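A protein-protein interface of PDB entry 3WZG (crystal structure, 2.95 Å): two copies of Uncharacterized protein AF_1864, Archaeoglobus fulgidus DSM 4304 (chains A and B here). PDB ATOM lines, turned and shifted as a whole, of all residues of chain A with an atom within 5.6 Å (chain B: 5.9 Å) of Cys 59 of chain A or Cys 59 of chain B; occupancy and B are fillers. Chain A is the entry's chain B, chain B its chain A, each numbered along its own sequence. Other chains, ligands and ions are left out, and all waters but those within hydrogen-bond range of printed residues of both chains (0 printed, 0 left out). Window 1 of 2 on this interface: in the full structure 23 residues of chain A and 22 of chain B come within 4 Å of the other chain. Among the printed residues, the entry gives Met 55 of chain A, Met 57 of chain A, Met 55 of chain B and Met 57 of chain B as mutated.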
ATOM      1  N   PRO A  54      12.631  25.213 -24.139  1.00  0.00           N
ATOM      2  CA  PRO A  54      12.384  23.831 -24.446  1.00  0.00           C
ATOM      3  C   PRO A  54      12.365  22.987 -23.186  1.00  0.00           C
ATOM      4  O   PRO A  54      12.978  23.379 -22.191  1.00  0.00           O
ATOM      5  CB  PRO A  54      13.577  23.451 -25.340  1.00  0.00           C
ATOM      6  CG  PRO A  54      14.652  24.388 -25.009  1.00  0.00           C
ATOM      7  CD  PRO A  54      14.004  25.631 -24.460  1.00  0.00           C
ATOM      8  N   MET A  55      11.736  21.815 -23.246  1.00  0.00           N
ATOM      9  CA  MET A  55      11.615  20.969 -22.063  1.00  0.00           C
ATOM     10  C   MET A  55      12.933  20.689 -21.447  1.00  0.00           C
ATOM     11  O   MET A  55      13.062  20.611 -20.223  1.00  0.00           O
ATOM     12  CB  MET A  55      10.923  19.620 -22.311  1.00  0.00           C
ATOM     13  CG  MET A  55       9.591  19.712 -23.090  1.00  0.00           C
ATOM     14  SD  MET A  55       8.100  20.600 -22.053  1.00  0.00           S
ATOM     15  CE  MET A  55       8.722  22.466 -21.774  1.00  0.00           C
ATOM     16  N   TRP A  56      13.956  20.603 -22.260  1.00  0.00           N
ATOM     17  CA  TRP A  56      15.245  20.234 -21.734  1.00  0.00           C
ATOM     18  C   TRP A  56      15.852  21.294 -20.867  1.00  0.00           C
ATOM     19  O   TRP A  56      16.523  20.994 -19.895  1.00  0.00           O
ATOM     20  CB  TRP A  56      16.220  19.807 -22.830  1.00  0.00           C
ATOM     21  CG  TRP A  56      16.313  20.610 -24.085  1.00  0.00           C
ATOM     22  CD1 TRP A  56      15.640  20.377 -25.247  1.00  0.00           C
ATOM     23  CD2 TRP A  56      17.207  21.671 -24.344  1.00  0.00           C
ATOM     24  NE1 TRP A  56      16.046  21.244 -26.198  1.00  0.00           N
ATOM     25  CE2 TRP A  56      17.004  22.062 -25.670  1.00  0.00           C
ATOM     26  CE3 TRP A  56      18.151  22.353 -23.577  1.00  0.00           C
ATOM     27  CZ2 TRP A  56      17.700  23.114 -26.257  1.00  0.00           C
ATOM     28  CZ3 TRP A  56      18.869  23.397 -24.167  1.00  0.00           C
ATOM     29  CH2 TRP A  56      18.632  23.766 -25.493  1.00  0.00           C
ATOM     30  N   MET A  57      15.612  22.536 -21.205  1.00  0.00           N
ATOM     31  CA  MET A  57      16.035  23.613 -20.341  1.00  0.00           C
ATOM     32  C   MET A  57      15.363  23.478 -19.013  1.00  0.00           C
ATOM     33  O   MET A  57      16.016  23.654 -17.988  1.00  0.00           O
ATOM     34  CB  MET A  57      15.649  24.943 -20.957  1.00  0.00           C
ATOM     35  CG  MET A  57      16.189  26.136 -20.167  1.00  0.00           C
ATOM     36  SD  MET A  57      18.128  26.119 -19.877  1.00  0.00           S
ATOM     37  CE  MET A  57      18.551  26.009 -21.792  1.00  0.00           C
ATOM     38  N   HIS A  58      14.054  23.212 -18.989  1.00  0.00           N
ATOM     39  CA  HIS A  58      13.375  23.174 -17.697  1.00  0.00           C
ATOM     40  C   HIS A  58      13.920  22.051 -16.859  1.00  0.00           C
ATOM     41  O   HIS A  58      14.290  22.257 -15.702  1.00  0.00           O
ATOM     42  CB  HIS A  58      11.900  22.980 -17.842  1.00  0.00           C
ATOM     43  CG  HIS A  58      11.175  24.177 -18.335  1.00  0.00           C
ATOM     44  ND1 HIS A  58      10.880  24.358 -19.671  1.00  0.00           N
ATOM     45  CD2 HIS A  58      10.618  25.220 -17.671  1.00  0.00           C
ATOM     46  CE1 HIS A  58      10.184  25.469 -19.816  1.00  0.00           C
ATOM     47  NE2 HIS A  58      10.033  26.020 -18.621  1.00  0.00           N
ATOM     48  N   CYS A  59      13.974  20.867 -17.446  1.00  0.00           N
ATOM     49  CA  CYS A  59      14.529  19.741 -16.746  1.00  0.00           C
ATOM     50  C   CYS A  59      15.966  19.983 -16.195  1.00  0.00           C
ATOM     51  O   CYS A  59      16.319  19.638 -15.054  1.00  0.00           O
ATOM     52  CB  CYS A  59      14.507  18.525 -17.660  1.00  0.00           C
ATOM     53  SG  CYS A  59      12.825  17.958 -18.060  1.00  0.00           S
ATOM     54  N   PHE A  60      16.788  20.577 -17.020  1.00  0.00           N
ATOM     55  CA  PHE A  60      18.145  20.810 -16.628  1.00  0.00           C
ATOM     56  C   PHE A  60      18.142  21.634 -15.374  1.00  0.00           C
ATOM     57  O   PHE A  60      18.804  21.290 -14.387  1.00  0.00           O
ATOM     58  CB  PHE A  60      18.863  21.531 -17.743  1.00  0.00           C
ATOM     59  CG  PHE A  60      20.164  22.106 -17.353  1.00  0.00           C
ATOM     60  CD1 PHE A  60      21.303  21.328 -17.321  1.00  0.00           C
ATOM     61  CD2 PHE A  60      20.270  23.456 -17.061  1.00  0.00           C
ATOM     62  CE1 PHE A  60      22.540  21.891 -17.005  1.00  0.00           C
ATOM     63  CE2 PHE A  60      21.488  24.023 -16.730  1.00  0.00           C
ATOM     64  CZ  PHE A  60      22.620  23.239 -16.708  1.00  0.00           C
ATOM     65  N   LEU A  61      17.394  22.723 -15.409  1.00  0.00           N
ATOM     66  CA  LEU A  61      17.405  23.639 -14.297  1.00  0.00           C
ATOM     67  C   LEU A  61      16.861  22.983 -13.052  1.00  0.00           C
ATOM     68  O   LEU A  61      17.360  23.199 -11.928  1.00  0.00           O
ATOM     69  CB  LEU A  61      16.596  24.873 -14.629  1.00  0.00           C
ATOM     70  CG  LEU A  61      17.243  25.823 -15.660  1.00  0.00           C
ATOM     71  CD1 LEU A  61      16.348  27.014 -15.959  1.00  0.00           C
ATOM     72  CD2 LEU A  61      18.581  26.358 -15.181  1.00  0.00           C
ATOM     73  N   ALA A  62      15.841  22.160 -13.236  1.00  0.00           N
ATOM     74  CA  ALA A  62      15.214  21.557 -12.090  1.00  0.00           C
ATOM     75  C   ALA A  62      16.192  20.636 -11.418  1.00  0.00           C
ATOM     76  O   ALA A  62      16.291  20.608 -10.210  1.00  0.00           O
ATOM     77  CB  ALA A  62      13.985  20.832 -12.516  1.00  0.00           C
ATOM     78  N   HIS A  63      16.958  19.893 -12.196  1.00  0.00           N
ATOM     79  CA  HIS A  63      17.940  19.003 -11.607  1.00  0.00           C
ATOM     80  C   HIS A  63      18.966  19.790 -10.813  1.00  0.00           C
ATOM     81  O   HIS A  63      19.456  19.346  -9.773  1.00  0.00           O
ATOM     82  CB  HIS A  63      18.643  18.222 -12.686  1.00  0.00           C
ATOM     83  CG  HIS A  63      19.936  17.617 -12.252  1.00  0.00           C
ATOM     84  ND1 HIS A  63      19.994  16.481 -11.462  1.00  0.00           N
ATOM     85  CD2 HIS A  63      21.215  17.979 -12.498  1.00  0.00           C
ATOM     86  CE1 HIS A  63      21.258  16.163 -11.246  1.00  0.00           C
ATOM     87  NE2 HIS A  63      22.020  17.063 -11.856  1.00  0.00           N
ATOM     88  N   LYS A  64      19.295  20.966 -11.297  1.00  0.00           N
ATOM     89  CA  LYS A  64      20.351  21.702 -10.673  1.00  0.00           C
ATOM     90  C   LYS A  64      19.965  22.204  -9.311  1.00  0.00           C
ATOM     91  O   LYS A  64      20.826  22.415  -8.489  1.00  0.00           O
ATOM     92  CB  LYS A  64      20.772  22.853 -11.536  1.00  0.00           C
ATOM     93  CG  LYS A  64      21.581  22.405 -12.743  1.00  0.00           C
ATOM     94  CD  LYS A  64      23.058  22.307 -12.437  1.00  0.00           C
ATOM     95  CE  LYS A  64      23.839  21.564 -13.506  1.00  0.00           C
ATOM     96  NZ  LYS A  64      24.666  20.459 -12.896  1.00  0.00           N
ATOM     97  N   VAL A  73       7.754  23.987 -10.712  1.00  0.00           N
ATOM     98  CA  VAL A  73       7.914  24.462 -12.049  1.00  0.00           C
ATOM     99  C   VAL A  73       6.649  25.237 -12.337  1.00  0.00           C
ATOM    100  O   VAL A  73       5.572  24.694 -12.164  1.00  0.00           O
ATOM    101  CB  VAL A  73       8.081  23.242 -12.963  1.00  0.00           C
ATOM    102  CG1 VAL A  73       8.045  23.654 -14.380  1.00  0.00           C
ATOM    103  CG2 VAL A  73       9.411  22.606 -12.718  1.00  0.00           C
ATOM    104  N   VAL A  83       7.772  19.081  -8.481  1.00  0.00           N
ATOM    105  CA  VAL A  83       8.165  17.918  -9.275  1.00  0.00           C
ATOM    106  C   VAL A  83       9.201  17.064  -8.607  1.00  0.00           C
ATOM    107  O   VAL A  83       9.453  15.962  -9.025  1.00  0.00           O
ATOM    108  CB  VAL A  83       8.742  18.329 -10.624  1.00  0.00           C
ATOM    109  CG1 VAL A  83       7.646  19.003 -11.458  1.00  0.00           C
ATOM    110  CG2 VAL A  83       9.952  19.256 -10.453  1.00  0.00           C
ATOM    111  N   PRO B  54       2.770  18.796 -20.328  1.00  0.00           N
ATOM    112  CA  PRO B  54       3.320  19.961 -19.660  1.00  0.00           C
ATOM    113  C   PRO B  54       4.728  19.724 -19.100  1.00  0.00           C
ATOM    114  O   PRO B  54       5.130  18.589 -18.872  1.00  0.00           O
ATOM    115  CB  PRO B  54       2.337  20.222 -18.534  1.00  0.00           C
ATOM    116  CG  PRO B  54       1.752  18.916 -18.230  1.00  0.00           C
ATOM    117  CD  PRO B  54       1.835  18.065 -19.480  1.00  0.00           C
ATOM    118  N   MET B  55       5.477  20.806 -18.912  1.00  0.00           N
ATOM    119  CA  MET B  55       6.870  20.647 -18.534  1.00  0.00           C
ATOM    120  C   MET B  55       6.994  19.910 -17.225  1.00  0.00           C
ATOM    121  O   MET B  55       8.009  19.206 -16.961  1.00  0.00           O
ATOM    122  CB  MET B  55       7.708  21.908 -18.554  1.00  0.00           C
ATOM    123  CG  MET B  55       7.750  22.543 -17.198  1.00  0.00           C
ATOM    124  SD  MET B  55       6.367  23.915 -17.102  1.00  0.00           S
ATOM    125  CE  MET B  55       4.571  23.142 -16.990  1.00  0.00           C
ATOM    126  N   TRP B  56       5.962  20.027 -16.404  1.00  0.00           N
ATOM    127  CA  TRP B  56       6.053  19.413 -15.119  1.00  0.00           C
ATOM    128  C   TRP B  56       6.067  17.893 -15.198  1.00  0.00           C
ATOM    129  O   TRP B  56       6.765  17.241 -14.430  1.00  0.00           O
ATOM    130  CB  TRP B  56       5.020  19.953 -14.167  1.00  0.00           C
ATOM    131  CG  TRP B  56       3.648  20.131 -14.621  1.00  0.00           C
ATOM    132  CD1 TRP B  56       3.064  21.289 -15.037  1.00  0.00           C
ATOM    133  CD2 TRP B  56       2.604  19.170 -14.547  1.00  0.00           C
ATOM    134  NE1 TRP B  56       1.735  21.098 -15.286  1.00  0.00           N
ATOM    135  CE2 TRP B  56       1.420  19.801 -14.985  1.00  0.00           C
ATOM    136  CE3 TRP B  56       2.555  17.830 -14.167  1.00  0.00           C
ATOM    137  CZ2 TRP B  56       0.231  19.143 -15.070  1.00  0.00           C
ATOM    138  CZ3 TRP B  56       1.361  17.178 -14.247  1.00  0.00           C
ATOM    139  CH2 TRP B  56       0.209  17.837 -14.694  1.00  0.00           C
ATOM    140  N   MET B  57       5.356  17.349 -16.180  1.00  0.00           N
ATOM    141  CA  MET B  57       5.431  15.940 -16.456  1.00  0.00           C
ATOM    142  C   MET B  57       6.826  15.537 -16.835  1.00  0.00           C
ATOM    143  O   MET B  57       7.357  14.569 -16.314  1.00  0.00           O
ATOM    144  CB  MET B  57       4.459  15.667 -17.588  1.00  0.00           C
ATOM    145  CG  MET B  57       4.347  14.157 -17.812  1.00  0.00           C
ATOM    146  SD  MET B  57       3.527  13.279 -16.225  1.00  0.00           S
ATOM    147  CE  MET B  57       4.802  11.857 -16.226  1.00  0.00           C
ATOM    148  N   HIS B  58       7.465  16.281 -17.726  1.00  0.00           N
ATOM    149  CA  HIS B  58       8.809  15.890 -18.151  1.00  0.00           C
ATOM    150  C   HIS B  58       9.803  15.952 -16.978  1.00  0.00           C
ATOM    151  O   HIS B  58      10.549  15.001 -16.733  1.00  0.00           O
ATOM    152  CB  HIS B  58       9.330  16.822 -19.241  1.00  0.00           C
ATOM    153  CG  HIS B  58       8.639  16.683 -20.568  1.00  0.00           C
ATOM    154  ND1 HIS B  58       7.516  17.407 -20.908  1.00  0.00           N
ATOM    155  CD2 HIS B  58       8.936  15.924 -21.646  1.00  0.00           C
ATOM    156  CE1 HIS B  58       7.130  17.072 -22.127  1.00  0.00           C
ATOM    157  NE2 HIS B  58       7.969  16.163 -22.585  1.00  0.00           N
ATOM    158  N   CYS B  59       9.807  17.081 -16.258  1.00  0.00           N
ATOM    159  CA  CYS B  59      10.675  17.230 -15.090  1.00  0.00           C
ATOM    160  C   CYS B  59      10.497  16.114 -14.047  1.00  0.00           C
ATOM    161  O   CYS B  59      11.448  15.535 -13.485  1.00  0.00           O
ATOM    162  CB  CYS B  59      10.439  18.581 -14.437  1.00  0.00           C
ATOM    163  SG  CYS B  59      10.919  19.987 -15.466  1.00  0.00           S
ATOM    164  N   PHE B  60       9.253  15.796 -13.794  1.00  0.00           N
ATOM    165  CA  PHE B  60       8.972  14.793 -12.819  1.00  0.00           C
ATOM    166  C   PHE B  60       9.621  13.494 -13.204  1.00  0.00           C
ATOM    167  O   PHE B  60      10.355  12.884 -12.404  1.00  0.00           O
ATOM    168  CB  PHE B  60       7.489  14.619 -12.750  1.00  0.00           C
ATOM    169  CG  PHE B  60       7.053  13.431 -12.005  1.00  0.00           C
ATOM    170  CD1 PHE B  60       6.974  13.464 -10.631  1.00  0.00           C
ATOM    171  CD2 PHE B  60       6.674  12.282 -12.683  1.00  0.00           C
ATOM    172  CE1 PHE B  60       6.516  12.344  -9.936  1.00  0.00           C
ATOM    173  CE2 PHE B  60       6.254  11.172 -11.995  1.00  0.00           C
ATOM    174  CZ  PHE B  60       6.167  11.208 -10.626  1.00  0.00           C
ATOM    175  N   LEU B  61       9.365  13.089 -14.429  1.00  0.00           N
ATOM    176  CA  LEU B  61       9.892  11.829 -14.891  1.00  0.00           C
ATOM    177  C   LEU B  61      11.422  11.831 -14.905  1.00  0.00           C
ATOM    178  O   LEU B  61      12.064  10.833 -14.536  1.00  0.00           O
ATOM    179  CB  LEU B  61       9.367  11.526 -16.284  1.00  0.00           C
ATOM    180  CG  LEU B  61       7.888  11.174 -16.381  1.00  0.00           C
ATOM    181  CD1 LEU B  61       7.465  10.953 -17.824  1.00  0.00           C
ATOM    182  CD2 LEU B  61       7.534   9.943 -15.589  1.00  0.00           C
ATOM    183  N   ALA B  62      12.013  12.960 -15.304  1.00  0.00           N
ATOM    184  CA  ALA B  62      13.447  13.022 -15.365  1.00  0.00           C
ATOM    185  C   ALA B  62      14.045  12.798 -13.987  1.00  0.00           C
ATOM    186  O   ALA B  62      15.000  12.065 -13.843  1.00  0.00           O
ATOM    187  CB  ALA B  62      13.901  14.363 -15.906  1.00  0.00           C
ATOM    188  N   HIS B  63      13.489  13.441 -12.978  1.00  0.00           N
ATOM    189  CA  HIS B  63      14.024  13.266 -11.673  1.00  0.00           C
ATOM    190  C   HIS B  63      13.954  11.786 -11.251  1.00  0.00           C
ATOM    191  O   HIS B  63      14.831  11.289 -10.534  1.00  0.00           O
ATOM    192  CB  HIS B  63      13.263  14.125 -10.678  1.00  0.00           C
ATOM    193  CG  HIS B  63      13.449  13.688  -9.268  1.00  0.00           C
ATOM    194  ND1 HIS B  63      14.599  13.943  -8.557  1.00  0.00           N
ATOM    195  CD2 HIS B  63      12.649  12.946  -8.461  1.00  0.00           C
ATOM    196  CE1 HIS B  63      14.496  13.399  -7.362  1.00  0.00           C
ATOM    197  NE2 HIS B  63      13.319  12.789  -7.274  1.00  0.00           N
ATOM    198  N   LYS B  64      12.904  11.096 -11.677  1.00  0.00           N
ATOM    199  CA  LYS B  64      12.666   9.774 -11.192  1.00  0.00           C
ATOM    200  C   LYS B  64      13.706   8.844 -11.718  1.00  0.00           C
ATOM    201  O   LYS B  64      14.000   7.858 -11.070  1.00  0.00           O
ATOM    202  CB  LYS B  64      11.284   9.281 -11.574  1.00  0.00           C
ATOM    203  CG  LYS B  64      10.170   9.927 -10.751  1.00  0.00           C
ATOM    204  CD  LYS B  64       9.870   9.168  -9.471  1.00  0.00           C
ATOM    205  CE  LYS B  64       9.030   9.978  -8.511  1.00  0.00           C
ATOM    206  NZ  LYS B  64       9.697  10.083  -7.168  1.00  0.00           N
ATOM    207  N   VAL B  73      16.196  14.160 -22.714  1.00  0.00           N
ATOM    208  CA  VAL B  73      14.862  14.599 -22.911  1.00  0.00           C
ATOM    209  C   VAL B  73      14.698  14.920 -24.364  1.00  0.00           C
ATOM    210  O   VAL B  73      15.479  15.666 -24.941  1.00  0.00           O
ATOM    211  CB  VAL B  73      14.663  15.837 -22.064  1.00  0.00           C
ATOM    212  CG1 VAL B  73      13.339  16.458 -22.342  1.00  0.00           C
ATOM    213  CG2 VAL B  73      14.721  15.481 -20.592  1.00  0.00           C
ATOM    214  N   VAL B  83      20.423  15.979 -19.875  1.00  0.00           N
ATOM    215  CA  VAL B  83      20.230  17.049 -18.922  1.00  0.00           C
ATOM    216  C   VAL B  83      20.895  16.758 -17.608  1.00  0.00           C
ATOM    217  O   VAL B  83      20.986  17.625 -16.788  1.00  0.00           O
ATOM    218  CB  VAL B  83      18.718  17.325 -18.703  1.00  0.00           C
ATOM    219  CG1 VAL B  83      18.084  17.896 -19.990  1.00  0.00           C
ATOM    220  CG2 VAL B  83      17.987  16.074 -18.235  1.00  0.00           C
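A ring nitrogen (ND1) of His 58 of chain B is in hydrogen-bond range of the side-chain sulfur (SD) of Met 55 of chain A, 3.4 Å away.
The backbone NH (N) of Cys 59 of chain B sits at hydrogen-bond distance from the side-chain sulfur (SG) of Cys 59 of chain A (3.6 Å).
Among the printed residues, pairs that only touch across the chains: Val 73 of chain A with Met 55 of chain B (3.0 Å), Met 55 of chain A with Met 55 of chain B (3.4 Å), Trp 56 of chain A with Val 83 of chain B (3.5 Å), Val 83 of chain A with Trp 56 of chain B (3.6 Å), Phe 60 of chain A with Val 83 of chain B (3.8 Å), Cys 59 of chain A with His 58 of chain B (3.8 Å), Val 83 of chain A with Phe 60 of chain B (3.9 Å), His 58 of chain A with Cys 59 of chain B (3.9 Å), His 58 of chain A with Met 55 of chain B (3.95 Å) and Met 55 of chain A with Val 73 of chain B (3.98 Å).
Met 55 of chain A touches His 58 of chain B, and with the chains exchanged His 58 of chain A touches Met 55 of chain B.
Met 55 of chain A touches Val 73 of chain B, and with the chains exchanged Val 73 of chain A touches Met 55 of chain B.
Trp 56 of chain A touches Val 83 of chain B, and with the chains exchanged Val 83 of chain A touches Trp 56 of chain B.
Cys 59 of chain A touches its own counterpart, Cys 59 of chain B.
Of the 12 pairs that touch across the chains among the printed residues, 12 have their exchanged pair printed and touching as well.
Of the printed residues of chain B, Cys 59 of chain A touches His 58 (3.8 Å) and Cys 59 (3.6 Å).
Printed residues of chain A within 4 Å of Val 73 of chain B: Met 55 (3.98 Å).
Printed residues of chain A within 4 Å of His 58 of chain B: Met 55 (3.4 Å) and Cys 59 (3.8 Å).
Pro 54 of chain A touches none of the printed residues of chain B.
O of Pro 54 of chain B sits at hydrogen-bond distance from ND1 of His 58 of chain B (3.4 Å).
The side-chain sulfur of Cys 59 of chain B lies within hydrogen-bond range of the backbone carbonyl oxygen of Met 55 of chain B.
ND1 of His 58 of chain A lies within hydrogen-bond range of O of Pro 54 of chain A (3.4 Å).
O of Met 55 of chain A sits at hydrogen-bond distance from SG of Cys 59 of chain A (3.4 Å).
Of the 13 printed residues of chain B, 7 touch a printed residue of chain A.
Printed residues of chain B that touch a printed residue of chain A: Met 55, Trp 56, His 58, Cys 59, Phe 60, Val 73 and Val 83.
Hydrophobic or aromatic side chains of chain B within 4 Å of the printed part of chain A: Met 55, Trp 56, His 58, Phe 60, Val 73 and Val 83.
Of the 13 printed residues of chain A, 7 touch a printed residue of chain B.
Hydrophobic or aromatic side chains of chain A that line the printed part of chain B: Met 55, Trp 56, His 58, Phe 60, Val 73 and Val 83.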
